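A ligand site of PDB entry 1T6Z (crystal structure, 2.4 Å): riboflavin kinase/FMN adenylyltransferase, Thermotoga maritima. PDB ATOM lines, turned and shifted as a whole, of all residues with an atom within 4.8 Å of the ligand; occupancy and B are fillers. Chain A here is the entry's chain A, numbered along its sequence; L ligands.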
ATOM      1  N   THR A 180      16.190  -1.802 -22.577  1.00  0.00           N
ATOM      2  CA  THR A 180      16.496  -0.527 -21.970  1.00  0.00           C
ATOM      3  C   THR A 180      17.288   0.285 -22.967  1.00  0.00           C
ATOM      4  O   THR A 180      18.218  -0.224 -23.610  1.00  0.00           O
ATOM      5  CB  THR A 180      17.351  -0.677 -20.698  1.00  0.00           C
ATOM      6  OG1 THR A 180      18.632  -1.227 -21.046  1.00  0.00           O
ATOM      7  CG2 THR A 180      16.649  -1.566 -19.702  1.00  0.00           C
ATOM      8  N   VAL A 197      17.151   3.442  -8.855  1.00  0.00           N
ATOM      9  CA  VAL A 197      16.050   3.367  -9.806  1.00  0.00           C
ATOM     10  C   VAL A 197      15.086   4.513  -9.661  1.00  0.00           C
ATOM     11  O   VAL A 197      14.725   4.913  -8.540  1.00  0.00           O
ATOM     12  CB  VAL A 197      15.284   2.034  -9.643  1.00  0.00           C
ATOM     13  CG1 VAL A 197      14.091   1.987 -10.563  1.00  0.00           C
ATOM     14  CG2 VAL A 197      16.221   0.904  -9.946  1.00  0.00           C
ATOM     15  N   VAL A 213      10.842   3.651 -16.262  1.00  0.00           N
ATOM     16  CA  VAL A 213      11.537   3.309 -15.035  1.00  0.00           C
ATOM     17  C   VAL A 213      12.985   3.410 -15.451  1.00  0.00           C
ATOM     18  O   VAL A 213      13.399   2.751 -16.409  1.00  0.00           O
ATOM     19  CB  VAL A 213      11.261   1.896 -14.567  1.00  0.00           C
ATOM     20  CG1 VAL A 213      11.963   1.668 -13.244  1.00  0.00           C
ATOM     21  CG2 VAL A 213       9.770   1.671 -14.416  1.00  0.00           C
ATOM     22  N   ASN A 215      17.100   3.290 -14.404  1.00  0.00           N
ATOM     23  CA  ASN A 215      18.084   2.850 -13.436  1.00  0.00           C
ATOM     24  C   ASN A 215      19.375   3.591 -13.698  1.00  0.00           C
ATOM     25  O   ASN A 215      19.769   3.783 -14.843  1.00  0.00           O
ATOM     26  CB  ASN A 215      18.286   1.332 -13.535  1.00  0.00           C
ATOM     27  CG  ASN A 215      19.456   0.856 -12.692  1.00  0.00           C
ATOM     28  OD1 ASN A 215      20.465   0.423 -13.236  1.00  0.00           O
ATOM     29  ND2 ASN A 215      19.333   0.958 -11.385  1.00  0.00           N
ATOM     30  N   LYS A 229      25.874   5.003 -15.844  1.00  0.00           N
ATOM     31  CA  LYS A 229      25.008   4.652 -16.960  1.00  0.00           C
ATOM     32  C   LYS A 229      23.523   4.955 -16.706  1.00  0.00           C
ATOM     33  O   LYS A 229      22.993   4.801 -15.595  1.00  0.00           O
ATOM     34  CB  LYS A 229      25.172   3.181 -17.343  1.00  0.00           C
ATOM     35  CG  LYS A 229      24.298   2.784 -18.529  1.00  0.00           C
ATOM     36  CD  LYS A 229      24.492   1.327 -18.938  1.00  0.00           C
ATOM     37  CE  LYS A 229      25.877   1.092 -19.527  1.00  0.00           C
ATOM     38  NZ  LYS A 229      25.935  -0.179 -20.321  1.00  0.00           N
ATOM     39  N   GLU A 231      19.880   3.967 -18.091  1.00  0.00           N
ATOM     40  CA  GLU A 231      19.054   3.076 -18.891  1.00  0.00           C
ATOM     41  C   GLU A 231      17.611   3.192 -18.470  1.00  0.00           C
ATOM     42  O   GLU A 231      17.289   3.218 -17.275  1.00  0.00           O
ATOM     43  CB  GLU A 231      19.535   1.640 -18.751  1.00  0.00           C
ATOM     44  CG  GLU A 231      20.743   1.301 -19.601  1.00  0.00           C
ATOM     45  CD  GLU A 231      21.348  -0.027 -19.221  1.00  0.00           C
ATOM     46  OE1 GLU A 231      22.199  -0.553 -19.965  1.00  0.00           O
ATOM     47  OE2 GLU A 231      20.973  -0.530 -18.143  1.00  0.00           O
ATOM     48  N   TYR A 233      13.476   1.812 -19.067  1.00  0.00           N
ATOM     49  CA  TYR A 233      12.498   0.871 -19.565  1.00  0.00           C
ATOM     50  C   TYR A 233      11.262   1.731 -19.744  1.00  0.00           C
ATOM     51  O   TYR A 233      10.645   2.176 -18.777  1.00  0.00           O
ATOM     52  CB  TYR A 233      12.224  -0.235 -18.536  1.00  0.00           C
ATOM     53  CG  TYR A 233      11.045  -1.094 -18.942  1.00  0.00           C
ATOM     54  CD1 TYR A 233      11.111  -1.916 -20.067  1.00  0.00           C
ATOM     55  CD2 TYR A 233       9.845  -1.038 -18.232  1.00  0.00           C
ATOM     56  CE1 TYR A 233      10.006  -2.658 -20.479  1.00  0.00           C
ATOM     57  CE2 TYR A 233       8.740  -1.786 -18.632  1.00  0.00           C
ATOM     58  CZ  TYR A 233       8.825  -2.588 -19.764  1.00  0.00           C
ATOM     59  OH  TYR A 233       7.725  -3.313 -20.168  1.00  0.00           O
ATOM     60  N   ARG A 255      14.161   2.983  -5.521  1.00  0.00           N
ATOM     61  CA  ARG A 255      14.999   2.142  -4.677  1.00  0.00           C
ATOM     62  C   ARG A 255      16.477   2.301  -5.042  1.00  0.00           C
ATOM     63  O   ARG A 255      16.804   2.629  -6.181  1.00  0.00           O
ATOM     64  CB  ARG A 255      14.618   0.673  -4.858  1.00  0.00           C
ATOM     65  CG  ARG A 255      15.081   0.071  -6.183  1.00  0.00           C
ATOM     66  CD  ARG A 255      14.519  -1.319  -6.376  1.00  0.00           C
ATOM     67  NE  ARG A 255      14.819  -1.888  -7.704  1.00  0.00           N
ATOM     68  CZ  ARG A 255      16.039  -2.204  -8.132  1.00  0.00           C
ATOM     69  NH1 ARG A 255      17.098  -2.016  -7.361  1.00  0.00           N
ATOM     70  NH2 ARG A 255      16.200  -2.730  -9.334  1.00  0.00           N
ATOM     71  N   ASP A 256      17.355   2.044  -4.068  1.00  0.00           N
ATOM     72  CA  ASP A 256      18.793   2.143  -4.304  1.00  0.00           C
ATOM     73  C   ASP A 256      19.242   1.001  -5.225  1.00  0.00           C
ATOM     74  O   ASP A 256      18.473   0.075  -5.491  1.00  0.00           O
ATOM     75  CB  ASP A 256      19.559   2.104  -2.984  1.00  0.00           C
ATOM     76  CG  ASP A 256      19.205   3.274  -2.067  1.00  0.00           C
ATOM     77  OD1 ASP A 256      18.099   3.252  -1.477  1.00  0.00           O
ATOM     78  OD2 ASP A 256      20.010   4.221  -1.941  1.00  0.00           O
ATOM     79  N   GLU A 257      20.474   1.083  -5.717  1.00  0.00           N
ATOM     80  CA  GLU A 257      21.010   0.065  -6.618  1.00  0.00           C
ATOM     81  C   GLU A 257      21.233  -1.256  -5.847  1.00  0.00           C
ATOM     82  O   GLU A 257      21.531  -1.229  -4.650  1.00  0.00           O
ATOM     83  CB  GLU A 257      22.316   0.536  -7.243  1.00  0.00           C
ATOM     84  CG  GLU A 257      22.820  -0.369  -8.356  1.00  0.00           C
ATOM     85  CD  GLU A 257      24.297  -0.181  -8.635  1.00  0.00           C
ATOM     86  OE1 GLU A 257      25.107  -0.289  -7.681  1.00  0.00           O
ATOM     87  OE2 GLU A 257      24.659   0.050  -9.815  1.00  0.00           O
ATOM     88  N   LYS A 258      21.113  -2.386  -6.545  1.00  0.00           N
ATOM     89  CA  LYS A 258      21.263  -3.703  -5.921  1.00  0.00           C
ATOM     90  C   LYS A 258      22.345  -4.595  -6.551  1.00  0.00           C
ATOM     91  O   LYS A 258      23.050  -4.171  -7.454  1.00  0.00           O
ATOM     92  CB  LYS A 258      19.908  -4.422  -5.970  1.00  0.00           C
ATOM     93  CG  LYS A 258      19.793  -5.673  -5.110  1.00  0.00           C
ATOM     94  CD  LYS A 258      18.369  -6.212  -5.147  1.00  0.00           C
ATOM     95  CE  LYS A 258      18.146  -7.263  -4.075  1.00  0.00           C
ATOM     96  NZ  LYS A 258      16.724  -7.711  -4.013  1.00  0.00           N
ATOM     97  N   LYS A 259      22.454  -5.824  -6.056  1.00  0.00           N
ATOM     98  CA  LYS A 259      23.430  -6.803  -6.554  1.00  0.00           C
ATOM     99  C   LYS A 259      23.357  -6.914  -8.066  1.00  0.00           C
ATOM    100  O   LYS A 259      22.816  -7.896  -8.586  1.00  0.00           O
ATOM    101  CB  LYS A 259      23.169  -8.178  -5.957  1.00  0.00           C
ATOM    102  CG  LYS A 259      23.313  -8.270  -4.459  1.00  0.00           C
ATOM    103  CD  LYS A 259      23.179  -9.723  -4.006  1.00  0.00           C
ATOM    104  CE  LYS A 259      23.483  -9.871  -2.525  1.00  0.00           C
ATOM    105  NZ  LYS A 259      23.455 -11.296  -2.108  1.00  0.00           N
ATOM    106  N   LEU A 266      17.399 -10.364 -10.891  1.00  0.00           N
ATOM    107  CA  LEU A 266      17.284  -9.011 -11.395  1.00  0.00           C
ATOM    108  C   LEU A 266      15.844  -8.812 -11.841  1.00  0.00           C
ATOM    109  O   LEU A 266      15.083  -8.076 -11.208  1.00  0.00           O
ATOM    110  CB  LEU A 266      18.226  -8.821 -12.577  1.00  0.00           C
ATOM    111  CG  LEU A 266      18.319  -7.414 -13.170  1.00  0.00           C
ATOM    112  CD1 LEU A 266      19.077  -6.515 -12.198  1.00  0.00           C
ATOM    113  CD2 LEU A 266      19.010  -7.462 -14.526  1.00  0.00           C
ATOM    114  N   ILE A 270      13.273  -5.613 -11.063  1.00  0.00           N
ATOM    115  CA  ILE A 270      13.009  -4.767 -12.217  1.00  0.00           C
ATOM    116  C   ILE A 270      11.680  -5.170 -12.836  1.00  0.00           C
ATOM    117  O   ILE A 270      11.443  -4.970 -14.017  1.00  0.00           O
ATOM    118  CB  ILE A 270      14.116  -4.875 -13.305  1.00  0.00           C
ATOM    119  CG1 ILE A 270      13.976  -6.174 -14.093  1.00  0.00           C
ATOM    120  CG2 ILE A 270      15.483  -4.820 -12.662  1.00  0.00           C
ATOM    121  CD1 ILE A 270      14.946  -6.285 -15.250  1.00  0.00           C
ATOM    122  N   ASP A 273       9.661  -2.764  -9.781  1.00  0.00           N
ATOM    123  CA  ASP A 273       9.898  -1.334  -9.995  1.00  0.00           C
ATOM    124  C   ASP A 273       8.828  -0.969 -11.013  1.00  0.00           C
ATOM    125  O   ASP A 273       8.103   0.006 -10.847  1.00  0.00           O
ATOM    126  CB  ASP A 273      11.275  -1.078 -10.609  1.00  0.00           C
ATOM    127  CG  ASP A 273      12.431  -1.479  -9.697  1.00  0.00           C
ATOM    128  OD1 ASP A 273      12.449  -1.043  -8.528  1.00  0.00           O
ATOM    129  OD2 ASP A 273      13.329  -2.219 -10.153  1.00  0.00           O
HETATM  130  N1  LIG L   1      21.457  -3.411 -12.170  1.00  0.00           N
HETATM  131  C1  LIG L   1      22.010  -3.517 -10.973  1.00  0.00           C
HETATM  132  O1  LIG L   1      23.133  -3.946 -10.815  1.00  0.00           O
HETATM  133  N2  LIG L   1      21.284  -3.108  -9.785  1.00  0.00           N
HETATM  134  C2  LIG L   1      19.997  -2.608  -9.832  1.00  0.00           C
HETATM  135  O2  LIG L   1      19.474  -2.304  -8.834  1.00  0.00           O
HETATM  136  C3  LIG L   1      19.353  -2.473 -11.147  1.00  0.00           C
HETATM  137  N3  LIG L   1      18.086  -1.972 -11.258  1.00  0.00           N
HETATM  138  C4  LIG L   1      17.527  -1.865 -12.502  1.00  0.00           C
HETATM  139  C5  LIG L   1      16.187  -1.330 -12.563  1.00  0.00           C
HETATM  140  C6  LIG L   1      15.530  -1.185 -13.794  1.00  0.00           C
HETATM  141  C7  LIG L   1      14.139  -0.617 -13.813  1.00  0.00           C
HETATM  142  C8  LIG L   1      16.212  -1.582 -15.046  1.00  0.00           C
HETATM  143  C9  LIG L   1      15.552  -1.455 -16.404  1.00  0.00           C
HETATM  144  C10 LIG L   1      17.534  -2.116 -15.000  1.00  0.00           C
HETATM  145  C11 LIG L   1      18.229  -2.271 -13.751  1.00  0.00           C
HETATM  146  N4  LIG L   1      19.598  -2.811 -13.583  1.00  0.00           N
HETATM  147  C12 LIG L   1      20.147  -2.912 -12.320  1.00  0.00           C
HETATM  148  C13 LIG L   1      20.509  -3.317 -14.745  1.00  0.00           C
HETATM  149  C14 LIG L   1      20.810  -2.530 -16.067  1.00  0.00           C
HETATM  150  O3  LIG L   1      19.630  -2.590 -16.828  1.00  0.00           O
HETATM  151  C15 LIG L   1      21.966  -3.211 -16.918  1.00  0.00           C
HETATM  152  O4  LIG L   1      21.610  -4.572 -17.219  1.00  0.00           O
HETATM  153  C16 LIG L   1      23.361  -3.192 -16.175  1.00  0.00           C
HETATM  154  O5  LIG L   1      23.760  -1.818 -15.860  1.00  0.00           O
HETATM  155  C17 LIG L   1      24.433  -3.858 -17.072  1.00  0.00           C
HETATM  156  O6  LIG L   1      25.864  -3.832 -16.294  1.00  0.00           O
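A nitrogen (N2) of the ligand is in hydrogen-bond range of the backbone carbonyl oxygen of Lys 258. N3 of the ligand lies within hydrogen-bond range of NH2 of Arg 255, 2.8 Å away. ND2 of Asn 215 lies within hydrogen-bond range of N3 of the ligand. O2 of the ligand lies within hydrogen-bond range of N of Lys 258 (2.8 Å). The side-chain carboxylate of Glu 231 sits at hydrogen-bond distance from an oxygen (O3) of the ligand, at 2.8 Å.
The backbone carbonyl oxygen (O) of Val 213 sits at hydrogen-bond distance from the backbone NH (N) of Tyr 233. The backbone NH (N) of Val 197 is in hydrogen-bond range of the backbone carbonyl oxygen (O) of Arg 255. The backbone NH of Asn 215 lies within hydrogen-bond range of the backbone carbonyl oxygen of Glu 231 (2.9 Å). OD1 of Asp 273 is in salt-bridge range of NE of Arg 255 (2.6 Å). OE1 of Glu 231 lies within salt-bridge range of NZ of Lys 229.
Residues that only touch the ligand: Val 213, Val 197, Glu 257, Thr 180, Ile 270, Leu 266 and Asp 273. The nearest printed residue that does not touch the ligand is Lys 259 (4.1 Å).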
